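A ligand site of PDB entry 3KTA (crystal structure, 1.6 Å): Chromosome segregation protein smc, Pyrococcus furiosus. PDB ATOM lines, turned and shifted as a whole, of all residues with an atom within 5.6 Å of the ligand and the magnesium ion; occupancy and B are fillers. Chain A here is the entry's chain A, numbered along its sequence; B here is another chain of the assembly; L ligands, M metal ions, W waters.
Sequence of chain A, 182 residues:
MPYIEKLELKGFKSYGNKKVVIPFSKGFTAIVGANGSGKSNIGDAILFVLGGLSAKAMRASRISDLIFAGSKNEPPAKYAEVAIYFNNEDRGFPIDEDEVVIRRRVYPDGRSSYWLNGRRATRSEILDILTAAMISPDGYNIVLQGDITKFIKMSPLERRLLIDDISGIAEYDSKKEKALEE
The backbone NH (N) of Ser 40 is in hydrogen-bond range of an oxygen (O13) of the ligand. An oxygen (O17) of the ligand sits at hydrogen-bond distance from the backbone NH (N) of Asn 173 of chain B. The chain-end carboxylate of Asn 173 of chain B sits at hydrogen-bond distance from an oxygen (O17) of the ligand (2.6 Å). An oxygen (O13) of the ligand sits at hydrogen-bond distance from the backbone NH of Asn 41 (2.7 Å). ND2 of Asn 41 lies within hydrogen-bond range of O20 of the ligand (3.0 Å). The guanidinium group (NH1) of Arg 59 lies within salt-bridge range of an oxygen (O14) of the ligand (2.8 Å). An oxygen (O10) of the ligand lies within hydrogen-bond range of the backbone NH (N) of Lys 39, at 2.9 Å. The side-chain amino group of Lys 39 lies within salt-bridge range of an oxygen (O10) of the ligand (2.9 Å). The backbone NH of Gly 36 lies within hydrogen-bond range of an oxygen (O9) of the ligand (2.9 Å). N of Gly 172 of chain B lies within hydrogen-bond range of O18 of the ligand (2.9 Å). The backbone carbonyl oxygen of Asp 65 is in hydrogen-bond range of a nitrogen (N8) of the ligand, at 3.0 Å. The backbone NH (N) of Gly 38 is in hydrogen-bond range of an oxygen (O10) of the ligand (3.1 Å). O of Ile 67 lies within hydrogen-bond range of N8 of the ligand. A nitrogen (N9) of the ligand is in hydrogen-bond range of the backbone NH of Ala 69. An oxygen (O10) of the ligand sits at hydrogen-bond distance from the backbone NH of Ser 37 (3.2 Å).
The side-chain amide oxygen (OD1) of Asn 173 of chain B sits close to the backbone carbonyl oxygen (O) of Glu 170 of chain B, 3.0 Å away. NH2 of Arg 59 sits at hydrogen-bond distance from OD1 of Asn 41. OD1 of Asn 41 sits close to NZ of Lys 13, 3.1 Å away. The side-chain amino group of Lys 39 lies within hydrogen-bond range of the backbone carbonyl oxygen of Ala 34 (3.0 Å). The side-chain amino group (NZ) of Lys 39 is in hydrogen-bond range of the backbone carbonyl oxygen (O) of Gly 33, 3.0 Å away. The backbone carbonyl oxygen (O) of Ser 37 sits at hydrogen-bond distance from the side-chain hydroxyl (OG) of Ser 146 of chain B (2.7 Å). N of Lys 13 sits at hydrogen-bond distance from O of Leu 66 (2.8 Å). N of Glu 94 of chain B lies within hydrogen-bond range of O of Ile 123 of chain B, at 2.8 Å.
A nitrogen (N9) of the ligand sits close to the backbone carbonyl oxygen of Lys 13 (3.3 Å). Ser 14 touches the ligand. Ala 34 touches the ligand (O to O10, 3.9 Å). CA of Asn 35 touches O7 of the ligand, 3.3 Å away. Leu 66 touches the ligand (C to N8, 3.98 Å). Phe 68 touches the ligand (CA to N9, 3.6 Å). OE1 of Glu 94 of chain B touches O8 of the ligand (3.6 Å). Met 141 of chain B touches the ligand. His 171 of chain B touches the ligand (CA to O18, 3.5 Å). Hydrophobic or aromatic side chains within 4 Å of the ligand: Phe 68, Met 141 of chain B and His 171 of chain B. Within 4 Å of the ligand: Lys 13, Ser 14, Ala 34, Asn 35, Gly 36, Ser 37, Gly 38, Lys 39, Ser 40, Asn 41, Arg 59, Asp 65, Leu 66, Ile 67, Phe 68, Ala 69, Gln 145, Glu 94 of chain B, Met 141 of chain B, His 171 of chain B, Gly 172 of chain B and Asn 173 of chain B. The nearest printed residue that does not touch the ligand is Glu 170 of chain B (4.4 Å).
Two residues have an atom within 4 Å of the magnesium ion: Ser 40 and Gln 145.
O8 of the ligand binds the magnesium ion, at 2.1 Å. The magnesium ion is bound by the side-chain amide oxygen (OE1) of Gln 145 (2.1 Å). The magnesium ion is bound by water W17, 2.1 Å away. The magnesium ion is bound by the side-chain hydroxyl (OG) of Ser 40 (2.1 Å). The magnesium ion is bound by O11 of the ligand, at 2.1 Å. Water W13 is bound to the magnesium ion, at 2.2 Å.
Water W13 bridges O14 of the ligand (2.7 Å) and NH1 of Arg 59 (3.3 Å). Water W17 lies within hydrogen-bond range of OE1 of Glu 94 of chain B and OD1 of Asp 93 of chain B. Water W6 lies within hydrogen-bond range of an oxygen (O21) of the ligand (2.6 Å) and the backbone carbonyl oxygen (O) of Gly 36 (2.7 Å). Water W2 lies within hydrogen-bond range of O3 of the ligand (2.7 Å) and NH1 of Arg 59 (3.3 Å). Water W10 lies within hydrogen-bond range of a nitrogen (N4) of the ligand and the backbone carbonyl oxygen (O) of Gln 145. Water W4 lies within hydrogen-bond range of O of Asp 65 (2.9 Å) and N7 of the ligand (2.9 Å).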
ATOM      1  N   LYS A  13     -35.267  24.102 -29.792  1.00  0.00           N
ATOM      2  CA  LYS A  13     -34.686  23.207 -28.781  1.00  0.00           C
ATOM      3  C   LYS A  13     -33.686  23.939 -27.875  1.00  0.00           C
ATOM      4  O   LYS A  13     -34.046  24.948 -27.263  1.00  0.00           O
ATOM      5  CB  LYS A  13     -34.101  21.946 -29.435  1.00  0.00           C
ATOM      6  CG  LYS A  13     -35.160  21.171 -30.218  1.00  0.00           C
ATOM      7  CD  LYS A  13     -34.679  19.812 -30.710  1.00  0.00           C
ATOM      8  CE  LYS A  13     -34.668  18.810 -29.583  1.00  0.00           C
ATOM      9  NZ  LYS A  13     -34.555  17.393 -30.041  1.00  0.00           N
ATOM     10  N   SER A  14     -32.458  23.449 -27.755  1.00  0.00           N
ATOM     11  CA  SER A  14     -31.515  24.054 -26.805  1.00  0.00           C
ATOM     12  C   SER A  14     -30.854  25.374 -27.259  1.00  0.00           C
ATOM     13  O   SER A  14     -29.995  25.911 -26.539  1.00  0.00           O
ATOM     14  CB  SER A  14     -30.416  23.046 -26.481  1.00  0.00           C
ATOM     15  OG  SER A  14     -29.724  22.664 -27.676  1.00  0.00           O
ATOM     16  N   GLY A  33     -18.252  18.620 -30.124  1.00  0.00           N
ATOM     17  CA  GLY A  33     -18.727  19.257 -28.900  1.00  0.00           C
ATOM     18  C   GLY A  33     -18.983  18.203 -27.844  1.00  0.00           C
ATOM     19  O   GLY A  33     -19.216  17.036 -28.155  1.00  0.00           O
ATOM     20  N   ALA A  34     -18.947  18.628 -26.584  1.00  0.00           N
ATOM     21  CA  ALA A  34     -19.106  17.725 -25.460  1.00  0.00           C
ATOM     22  C   ALA A  34     -20.425  16.962 -25.526  1.00  0.00           C
ATOM     23  O   ALA A  34     -21.398  17.417 -26.140  1.00  0.00           O
ATOM     24  CB  ALA A  34     -19.016  18.507 -24.159  1.00  0.00           C
ATOM     25  N   ASN A  35     -20.457  15.797 -24.888  1.00  0.00           N
ATOM     26  CA  ASN A  35     -21.707  15.078 -24.731  1.00  0.00           C
ATOM     27  C   ASN A  35     -22.777  16.005 -24.159  1.00  0.00           C
ATOM     28  O   ASN A  35     -22.530  16.737 -23.213  1.00  0.00           O
ATOM     29  CB  ASN A  35     -21.495  13.911 -23.761  1.00  0.00           C
ATOM     30  CG  ASN A  35     -20.388  12.974 -24.195  1.00  0.00           C
ATOM     31  OD1 ASN A  35     -20.615  11.788 -24.404  1.00  0.00           O
ATOM     32  ND2 ASN A  35     -19.168  13.492 -24.332  1.00  0.00           N
ATOM     33  N   GLY A  36     -23.972  15.975 -24.748  1.00  0.00           N
ATOM     34  CA  GLY A  36     -25.073  16.797 -24.275  1.00  0.00           C
ATOM     35  C   GLY A  36     -25.025  18.276 -24.633  1.00  0.00           C
ATOM     36  O   GLY A  36     -25.859  19.064 -24.166  1.00  0.00           O
ATOM     37  N   SER A  37     -24.083  18.665 -25.487  1.00  0.00           N
ATOM     38  CA  SER A  37     -23.900  20.089 -25.776  1.00  0.00           C
ATOM     39  C   SER A  37     -24.927  20.673 -26.756  1.00  0.00           C
ATOM     40  O   SER A  37     -25.081  21.900 -26.819  1.00  0.00           O
ATOM     41  CB  SER A  37     -22.493  20.376 -26.288  1.00  0.00           C
ATOM     42  OG  SER A  37     -22.237  19.607 -27.446  1.00  0.00           O
ATOM     43  N   GLY A  38     -25.618  19.796 -27.493  1.00  0.00           N
ATOM     44  CA  GLY A  38     -26.627  20.225 -28.462  1.00  0.00           C
ATOM     45  C   GLY A  38     -26.374  19.852 -29.927  1.00  0.00           C
ATOM     46  O   GLY A  38     -26.963  20.453 -30.834  1.00  0.00           O
ATOM     47  N   LYS A  39     -25.510  18.865 -30.172  1.00  0.00           N
ATOM     48  CA  LYS A  39     -25.129  18.518 -31.544  1.00  0.00           C
ATOM     49  C   LYS A  39     -26.290  17.896 -32.341  1.00  0.00           C
ATOM     50  O   LYS A  39     -26.626  18.359 -33.453  1.00  0.00           O
ATOM     51  CB  LYS A  39     -23.902  17.592 -31.544  1.00  0.00           C
ATOM     52  CG  LYS A  39     -22.684  18.211 -30.841  1.00  0.00           C
ATOM     53  CD  LYS A  39     -21.492  17.238 -30.882  1.00  0.00           C
ATOM     54  CE  LYS A  39     -21.812  15.887 -30.242  1.00  0.00           C
ATOM     55  NZ  LYS A  39     -21.934  15.960 -28.757  1.00  0.00           N
ATOM     56  N   SER A  40     -26.913  16.862 -31.788  1.00  0.00           N
ATOM     57  CA  SER A  40     -27.981  16.196 -32.515  1.00  0.00           C
ATOM     58  C   SER A  40     -29.161  17.129 -32.770  1.00  0.00           C
ATOM     59  O   SER A  40     -29.895  16.937 -33.738  1.00  0.00           O
ATOM     60  CB  SER A  40     -28.470  14.960 -31.777  1.00  0.00           C
ATOM     61  OG  SER A  40     -27.429  14.002 -31.729  1.00  0.00           O
ATOM     62  N   ASN A  41     -29.357  18.095 -31.896  1.00  0.00           N
ATOM     63  CA  ASN A  41     -30.424  19.090 -32.097  1.00  0.00           C
ATOM     64  C   ASN A  41     -30.291  19.842 -33.430  1.00  0.00           C
ATOM     65  O   ASN A  41     -31.287  20.295 -33.998  1.00  0.00           O
ATOM     66  CB  ASN A  41     -30.475  20.083 -30.924  1.00  0.00           C
ATOM     67  CG  ASN A  41     -31.046  19.465 -29.663  1.00  0.00           C
ATOM     68  OD1 ASN A  41     -31.641  18.382 -29.689  1.00  0.00           O
ATOM     69  ND2 ASN A  41     -30.873  20.167 -28.549  1.00  0.00           N
ATOM     70  N   ILE A  42     -29.062  20.016 -33.920  1.00  0.00           N
ATOM     71  CA  ILE A  42     -28.854  20.602 -35.254  1.00  0.00           C
ATOM     72  C   ILE A  42     -29.436  19.707 -36.342  1.00  0.00           C
ATOM     73  O   ILE A  42     -30.098  20.178 -37.260  1.00  0.00           O
ATOM     74  CB  ILE A  42     -27.364  20.872 -35.524  1.00  0.00           C
ATOM     75  CG1 ILE A  42     -26.812  21.857 -34.486  1.00  0.00           C
ATOM     76  CG2 ILE A  42     -27.157  21.363 -36.956  1.00  0.00           C
ATOM     77  CD1 ILE A  42     -25.310  22.072 -34.620  1.00  0.00           C
ATOM     78  N   ARG A  59     -37.207  13.418 -30.937  1.00  0.00           N
ATOM     79  CA  ARG A  59     -37.087  13.197 -29.498  1.00  0.00           C
ATOM     80  C   ARG A  59     -37.946  14.162 -28.684  1.00  0.00           C
ATOM     81  O   ARG A  59     -37.552  14.600 -27.595  1.00  0.00           O
ATOM     82  CB  ARG A  59     -35.624  13.248 -29.063  1.00  0.00           C
ATOM     83  CG  ARG A  59     -34.811  12.113 -29.660  1.00  0.00           C
ATOM     84  CD  ARG A  59     -33.344  12.285 -29.374  1.00  0.00           C
ATOM     85  NE  ARG A  59     -32.829  13.472 -30.068  1.00  0.00           N
ATOM     86  CZ  ARG A  59     -31.948  14.311 -29.546  1.00  0.00           C
ATOM     87  NH1 ARG A  59     -31.458  14.117 -28.329  1.00  0.00           N
ATOM     88  NH2 ARG A  59     -31.554  15.361 -30.264  1.00  0.00           N
ATOM     89  N   ASP A  65     -43.020  20.813 -28.058  1.00  0.00           N
ATOM     90  CA  ASP A  65     -41.936  20.566 -27.114  1.00  0.00           C
ATOM     91  C   ASP A  65     -40.581  20.950 -27.714  1.00  0.00           C
ATOM     92  O   ASP A  65     -39.569  20.958 -27.019  1.00  0.00           O
ATOM     93  CB  ASP A  65     -41.898  19.098 -26.695  1.00  0.00           C
ATOM     94  CG  ASP A  65     -43.067  18.719 -25.781  1.00  0.00           C
ATOM     95  OD1 ASP A  65     -43.566  19.597 -25.051  1.00  0.00           O
ATOM     96  OD2 ASP A  65     -43.472  17.540 -25.799  1.00  0.00           O
ATOM     97  N   LEU A  66     -40.583  21.248 -29.010  1.00  0.00           N
ATOM     98  CA  LEU A  66     -39.376  21.713 -29.687  1.00  0.00           C
ATOM     99  C   LEU A  66     -39.077  23.173 -29.382  1.00  0.00           C
ATOM    100  O   LEU A  66     -38.032  23.706 -29.766  1.00  0.00           O
ATOM    101  CB  LEU A  66     -39.535  21.524 -31.193  1.00  0.00           C
ATOM    102  CG  LEU A  66     -39.633  20.092 -31.711  1.00  0.00           C
ATOM    103  CD1 LEU A  66     -39.842  20.114 -33.216  1.00  0.00           C
ATOM    104  CD2 LEU A  66     -38.375  19.305 -31.356  1.00  0.00           C
ATOM    105  N   ILE A  67     -40.003  23.850 -28.711  1.00  0.00           N
ATOM    106  CA  ILE A  67     -39.800  25.256 -28.412  1.00  0.00           C
ATOM    107  C   ILE A  67     -38.885  25.418 -27.208  1.00  0.00           C
ATOM    108  O   ILE A  67     -39.103  24.797 -26.170  1.00  0.00           O
ATOM    109  CB  ILE A  67     -41.139  25.988 -28.174  1.00  0.00           C
ATOM    110  CG1 ILE A  67     -41.996  25.896 -29.429  1.00  0.00           C
ATOM    111  CG2 ILE A  67     -40.872  27.425 -27.815  1.00  0.00           C
ATOM    112  CD1 ILE A  67     -43.400  26.494 -29.266  1.00  0.00           C
ATOM    113  N   PHE A  68     -37.863  26.247 -27.394  1.00  0.00           N
ATOM    114  CA  PHE A  68     -36.892  26.539 -26.348  1.00  0.00           C
ATOM    115  C   PHE A  68     -37.534  26.910 -25.026  1.00  0.00           C
ATOM    116  O   PHE A  68     -38.344  27.826 -24.941  1.00  0.00           O
ATOM    117  CB  PHE A  68     -35.962  27.654 -26.763  1.00  0.00           C
ATOM    118  CG  PHE A  68     -35.045  28.099 -25.672  1.00  0.00           C
ATOM    119  CD1 PHE A  68     -34.041  27.263 -25.206  1.00  0.00           C
ATOM    120  CD2 PHE A  68     -35.179  29.367 -25.103  1.00  0.00           C
ATOM    121  CE1 PHE A  68     -33.171  27.676 -24.199  1.00  0.00           C
ATOM    122  CE2 PHE A  68     -34.318  29.778 -24.098  1.00  0.00           C
ATOM    123  CZ  PHE A  68     -33.321  28.933 -23.641  1.00  0.00           C
ATOM    124  N   ALA A  69     -37.140  26.175 -23.987  1.00  0.00           N
ATOM    125  CA  ALA A  69     -37.495  26.494 -22.618  1.00  0.00           C
ATOM    126  C   ALA A  69     -36.277  26.125 -21.797  1.00  0.00           C
ATOM    127  O   ALA A  69     -35.977  24.942 -21.638  1.00  0.00           O
ATOM    128  CB  ALA A  69     -38.690  25.693 -22.197  1.00  0.00           C
ATOM    129  N   GLY A  70     -35.543  27.122 -21.317  1.00  0.00           N
ATOM    130  CA  GLY A  70     -34.312  26.907 -20.580  1.00  0.00           C
ATOM    131  C   GLY A  70     -34.477  26.049 -19.345  1.00  0.00           C
ATOM    132  O   GLY A  70     -33.652  25.170 -19.082  1.00  0.00           O
ATOM    133  N   GLN A 145     -28.670   9.509 -34.809  1.00  0.00           N
ATOM    134  CA  GLN A 145     -27.798   8.891 -33.817  1.00  0.00           C
ATOM    135  C   GLN A 145     -28.271   7.484 -33.475  1.00  0.00           C
ATOM    136  O   GLN A 145     -29.461   7.256 -33.212  1.00  0.00           O
ATOM    137  CB  GLN A 145     -27.725   9.762 -32.577  1.00  0.00           C
ATOM    138  CG  GLN A 145     -26.685   9.249 -31.565  1.00  0.00           C
ATOM    139  CD  GLN A 145     -26.307  10.315 -30.545  1.00  0.00           C
ATOM    140  OE1 GLN A 145     -26.759  11.448 -30.615  1.00  0.00           O
ATOM    141  NE2 GLN A 145     -25.473   9.942 -29.575  1.00  0.00           N
ATOM    142  N   GLY A 146     -27.344   6.531 -33.506  1.00  0.00           N
ATOM    143  CA  GLY A 146     -27.651   5.146 -33.170  1.00  0.00           C
ATOM    144  C   GLY A 146     -28.375   4.347 -34.246  1.00  0.00           C
ATOM    145  O   GLY A 146     -28.755   3.201 -33.993  1.00  0.00           O
ATOM    146  N   ASP B  93     -24.919  11.130 -37.775  1.00  0.00           N
ATOM    147  CA  ASP B  93     -24.746  11.458 -36.351  1.00  0.00           C
ATOM    148  C   ASP B  93     -24.060  10.328 -35.566  1.00  0.00           C
ATOM    149  O   ASP B  93     -24.686   9.320 -35.248  1.00  0.00           O
ATOM    150  CB  ASP B  93     -26.121  11.742 -35.750  1.00  0.00           C
ATOM    151  CG  ASP B  93     -26.053  12.410 -34.387  1.00  0.00           C
ATOM    152  OD1 ASP B  93     -24.971  12.408 -33.752  1.00  0.00           O
ATOM    153  OD2 ASP B  93     -27.094  12.951 -33.955  1.00  0.00           O
ATOM    154  N   GLU B  94     -22.775  10.506 -35.267  1.00  0.00           N
ATOM    155  CA  GLU B  94     -21.974   9.531 -34.523  1.00  0.00           C
ATOM    156  C   GLU B  94     -22.066   8.109 -35.107  1.00  0.00           C
ATOM    157  O   GLU B  94     -22.278   7.132 -34.405  1.00  0.00           O
ATOM    158  CB  GLU B  94     -22.270   9.605 -33.015  1.00  0.00           C
ATOM    159  CG  GLU B  94     -21.956  10.958 -32.445  1.00  0.00           C
ATOM    160  CD  GLU B  94     -21.987  11.007 -30.938  1.00  0.00           C
ATOM    161  OE1 GLU B  94     -22.571  11.968 -30.400  1.00  0.00           O
ATOM    162  OE2 GLU B  94     -21.411  10.097 -30.283  1.00  0.00           O
ATOM    163  N   ILE B 123     -21.620  14.536 -37.349  1.00  0.00           N
ATOM    164  CA  ILE B 123     -21.391  14.774 -35.933  1.00  0.00           C
ATOM    165  C   ILE B 123     -20.492  13.666 -35.401  1.00  0.00           C
ATOM    166  O   ILE B 123     -20.767  12.493 -35.635  1.00  0.00           O
ATOM    167  CB  ILE B 123     -22.696  14.741 -35.158  1.00  0.00           C
ATOM    168  CG1 ILE B 123     -23.618  15.881 -35.619  1.00  0.00           C
ATOM    169  CG2 ILE B 123     -22.397  14.842 -33.658  1.00  0.00           C
ATOM    170  CD1 ILE B 123     -25.083  15.706 -35.220  1.00  0.00           C
ATOM    171  N   MET B 141     -22.428  24.076 -24.469  1.00  0.00           N
ATOM    172  CA  MET B 141     -23.580  24.511 -23.690  1.00  0.00           C
ATOM    173  C   MET B 141     -23.156  25.312 -22.472  1.00  0.00           C
ATOM    174  O   MET B 141     -22.255  24.913 -21.739  1.00  0.00           O
ATOM    175  CB  MET B 141     -24.419  23.314 -23.260  1.00  0.00           C
ATOM    176  CG  MET B 141     -25.629  23.734 -22.452  1.00  0.00           C
ATOM    177  SD  MET B 141     -26.840  22.301 -22.150  1.00  0.00           S
ATOM    178  CE  MET B 141     -27.483  22.053 -23.998  1.00  0.00           C
ATOM    179  N   GLY B 144     -27.480  26.246 -19.789  1.00  0.00           N
ATOM    180  CA  GLY B 144     -28.590  25.554 -20.428  1.00  0.00           C
ATOM    181  C   GLY B 144     -28.802  25.833 -21.902  1.00  0.00           C
ATOM    182  O   GLY B 144     -29.726  25.302 -22.500  1.00  0.00           O
ATOM    183  N   SER B 146     -27.292  26.116 -25.934  1.00  0.00           N
ATOM    184  CA  SER B 146     -26.270  25.690 -26.893  1.00  0.00           C
ATOM    185  C   SER B 146     -25.831  26.876 -27.728  1.00  0.00           C
ATOM    186  O   SER B 146     -26.628  27.760 -28.021  1.00  0.00           O
ATOM    187  CB  SER B 146     -26.813  24.619 -27.842  1.00  0.00           C
ATOM    188  OG  SER B 146     -27.226  23.455 -27.151  1.00  0.00           O
ATOM    189  N   GLU B 170     -18.151   7.633 -25.328  1.00  0.00           N
ATOM    190  CA  GLU B 170     -18.695   7.042 -26.558  1.00  0.00           C
ATOM    191  C   GLU B 170     -20.206   6.874 -26.530  1.00  0.00           C
ATOM    192  O   GLU B 170     -20.800   6.621 -25.488  1.00  0.00           O
ATOM    193  CB  GLU B 170     -18.012   5.708 -26.884  1.00  0.00           C
ATOM    194  CG  GLU B 170     -18.366   5.155 -28.256  1.00  0.00           C
ATOM    195  CD  GLU B 170     -17.495   3.977 -28.660  1.00  0.00           C
ATOM    196  OE1 GLU B 170     -17.127   3.180 -27.761  1.00  0.00           O
ATOM    197  OE2 GLU B 170     -17.199   3.824 -29.860  1.00  0.00           O
ATOM    198  N   HIS B 171     -20.823   7.036 -27.690  1.00  0.00           N
ATOM    199  CA  HIS B 171     -22.250   6.788 -27.850  1.00  0.00           C
ATOM    200  C   HIS B 171     -22.631   5.406 -27.321  1.00  0.00           C
ATOM    201  O   HIS B 171     -21.898   4.423 -27.509  1.00  0.00           O
ATOM    202  CB  HIS B 171     -22.643   6.869 -29.328  1.00  0.00           C
ATOM    203  CG  HIS B 171     -24.023   6.367 -29.611  1.00  0.00           C
ATOM    204  ND1 HIS B 171     -24.297   5.073 -29.975  1.00  0.00           N
ATOM    205  CD2 HIS B 171     -25.223   6.995 -29.519  1.00  0.00           C
ATOM    206  CE1 HIS B 171     -25.596   4.919 -30.118  1.00  0.00           C
ATOM    207  NE2 HIS B 171     -26.187   6.066 -29.844  1.00  0.00           N
ATOM    208  N   GLY B 172     -23.774   5.327 -26.656  1.00  0.00           N
ATOM    209  CA  GLY B 172     -24.304   4.054 -26.207  1.00  0.00           C
ATOM    210  C   GLY B 172     -24.029   3.735 -24.754  1.00  0.00           C
ATOM    211  O   GLY B 172     -24.497   2.717 -24.240  1.00  0.00           O
ATOM    212  N   ASN B 173     -23.252   4.587 -24.086  1.00  0.00           N
ATOM    213  CA  ASN B 173     -22.901   4.359 -22.689  1.00  0.00           C
ATOM    214  C   ASN B 173     -23.938   4.873 -21.717  1.00  0.00           C
ATOM    215  O   ASN B 173     -24.789   5.689 -22.084  1.00  0.00           O
ATOM    216  CB  ASN B 173     -21.540   4.968 -22.353  1.00  0.00           C
ATOM    217  CG  ASN B 173     -20.386   4.139 -22.862  1.00  0.00           C
ATOM    218  OD1 ASN B 173     -19.558   4.621 -23.651  1.00  0.00           O
ATOM    219  ND2 ASN B 173     -20.316   2.877 -22.433  1.00  0.00           N
ATOM    220  OXT ASN B 173     -23.928   4.467 -20.552  1.00  0.00           O
HETATM  221  P1  LIG L   1     -28.445  11.304 -23.251  1.00  0.00           P
HETATM  222  O1  LIG L   1     -27.779  11.571 -21.919  1.00  0.00           O
HETATM  223  O2  LIG L   1     -29.928  11.521 -23.215  1.00  0.00           O
HETATM  224  O3  LIG L   1     -27.862  12.269 -24.423  1.00  0.00           O
HETATM  225  P2  LIG L   1     -26.336  12.681 -24.553  1.00  0.00           P
HETATM  226  O4  LIG L   1     -25.450  11.510 -24.173  1.00  0.00           O
HETATM  227  O5  LIG L   1     -26.026  13.967 -23.820  1.00  0.00           O
HETATM  228  O6  LIG L   1     -26.456  12.892 -26.140  1.00  0.00           O
HETATM  229  P3  LIG L   1     -25.287  13.499 -26.980  1.00  0.00           P
HETATM  230  O7  LIG L   1     -23.969  13.263 -26.244  1.00  0.00           O
HETATM  231  O8  LIG L   1     -25.341  12.830 -28.316  1.00  0.00           O
HETATM  232  O9  LIG L   1     -25.612  15.040 -26.920  1.00  0.00           O
HETATM  233  P4  LIG L   1     -25.822  16.079 -28.103  1.00  0.00           P
HETATM  234  O10 LIG L   1     -24.624  16.982 -28.203  1.00  0.00           O
HETATM  235  O11 LIG L   1     -26.235  15.425 -29.397  1.00  0.00           O
HETATM  236  O12 LIG L   1     -27.018  16.935 -27.453  1.00  0.00           O
HETATM  237  P5  LIG L   1     -28.530  17.056 -28.030  1.00  0.00           P
HETATM  238  O13 LIG L   1     -28.441  17.760 -29.370  1.00  0.00           O
HETATM  239  O14 LIG L   1     -29.224  15.744 -27.995  1.00  0.00           O
HETATM  240  O15 LIG L   1     -28.048   9.848 -23.807  1.00  0.00           O
HETATM  241  C1  LIG L   1     -28.704   8.651 -23.435  1.00  0.00           C
HETATM  242  C2  LIG L   1     -28.094   7.424 -24.123  1.00  0.00           C
HETATM  243  O16 LIG L   1     -28.505   7.401 -25.480  1.00  0.00           O
HETATM  244  C3  LIG L   1     -26.571   7.448 -24.157  1.00  0.00           C
HETATM  245  O17 LIG L   1     -26.093   6.129 -24.314  1.00  0.00           O
HETATM  246  C4  LIG L   1     -26.285   8.201 -25.439  1.00  0.00           C
HETATM  247  O18 LIG L   1     -25.038   7.841 -25.991  1.00  0.00           O
HETATM  248  C5  LIG L   1     -27.448   7.787 -26.331  1.00  0.00           C
HETATM  249  N1  LIG L   1     -27.962   8.910 -27.131  1.00  0.00           N
HETATM  250  C6  LIG L   1     -27.741  10.244 -26.935  1.00  0.00           C
HETATM  251  N2  LIG L   1     -28.426  10.931 -27.882  1.00  0.00           N
HETATM  252  C7  LIG L   1     -29.069  10.049 -28.678  1.00  0.00           C
HETATM  253  C8  LIG L   1     -29.889  10.221 -29.787  1.00  0.00           C
HETATM  254  N3  LIG L   1     -30.057  11.427 -30.326  1.00  0.00           N
HETATM  255  N4  LIG L   1     -30.411   9.099 -30.404  1.00  0.00           N
HETATM  256  C9  LIG L   1     -30.125   7.837 -29.926  1.00  0.00           C
HETATM  257  N5  LIG L   1     -29.304   7.671 -28.825  1.00  0.00           N
HETATM  258  C10 LIG L   1     -28.787   8.769 -28.214  1.00  0.00           C
HETATM  259  O19 LIG L   1     -29.085  18.121 -26.962  1.00  0.00           O
HETATM  260  C11 LIG L   1     -29.588  17.695 -25.707  1.00  0.00           C
HETATM  261  C12 LIG L   1     -29.925  18.943 -24.919  1.00  0.00           C
HETATM  262  O20 LIG L   1     -30.947  19.663 -25.605  1.00  0.00           O
HETATM  263  C13 LIG L   1     -30.474  18.600 -23.533  1.00  0.00           C
HETATM  264  O21 LIG L   1     -29.833  19.407 -22.579  1.00  0.00           O
HETATM  265  C14 LIG L   1     -31.926  18.981 -23.659  1.00  0.00           C
HETATM  266  O22 LIG L   1     -32.521  19.308 -22.413  1.00  0.00           O
HETATM  267  C15 LIG L   1     -31.861  20.136 -24.643  1.00  0.00           C
HETATM  268  N6  LIG L   1     -33.203  20.408 -25.191  1.00  0.00           N
HETATM  269  C16 LIG L   1     -33.994  19.619 -25.990  1.00  0.00           C
HETATM  270  N7  LIG L   1     -35.152  20.277 -26.224  1.00  0.00           N
HETATM  271  C17 LIG L   1     -35.100  21.469 -25.568  1.00  0.00           C
HETATM  272  C18 LIG L   1     -35.991  22.520 -25.444  1.00  0.00           C
HETATM  273  N8  LIG L   1     -37.224  22.422 -25.939  1.00  0.00           N
HETATM  274  N9  LIG L   1     -35.626  23.612 -24.698  1.00  0.00           N
HETATM  275  C19 LIG L   1     -34.407  23.680 -24.062  1.00  0.00           C
HETATM  276  N10 LIG L   1     -33.526  22.622 -24.181  1.00  0.00           N
HETATM  277  C20 LIG L   1     -33.877  21.554 -24.919  1.00  0.00           C
HETATM  278 MG    MG M   1     -26.369  13.404 -30.017  1.00  0.00          MG
HETATM  279  O   HOH W   1     -22.071  13.281 -28.114  1.00  0.00           O
HETATM  280  O   HOH W   2     -29.629  13.946 -25.552  1.00  0.00           O
HETATM  281  O   HOH W   3     -28.182  15.641 -22.715  1.00  0.00           O
HETATM  282  O   HOH W   4     -37.446  19.077 -27.474  1.00  0.00           O
HETATM  283  O   HOH W   5     -30.948   9.076 -26.048  1.00  0.00           O
HETATM  284  O   HOH W   6     -27.519  18.233 -22.257  1.00  0.00           O
HETATM  285  O   HOH W   7     -27.869   4.226 -25.725  1.00  0.00           O
HETATM  286  O   HOH W   8     -35.178  18.916 -22.556  1.00  0.00           O
HETATM  287  O   HOH W   9     -29.509   5.073 -27.737  1.00  0.00           O
HETATM  288  O   HOH W  10     -31.940   8.903 -32.829  1.00  0.00           O
HETATM  289  O   HOH W  11     -23.177  10.699 -23.541  1.00  0.00           O
HETATM  290  O   HOH W  12     -25.153  14.110 -21.379  1.00  0.00           O
HETATM  291  O   HOH W  13     -28.275  13.413 -28.940  1.00  0.00           O
HETATM  292  O   HOH W  14     -24.000  10.256 -26.700  1.00  0.00           O
HETATM  293  O   HOH W  15     -25.936  10.425 -20.535  1.00  0.00           O
HETATM  294  O   HOH W  16     -31.380  11.585 -32.992  1.00  0.00           O
HETATM  295  O   HOH W  17     -24.644  13.455 -31.191  1.00  0.00           O
HETATM  296  O   HOH W  18     -30.760  14.546 -22.940  1.00  0.00           O
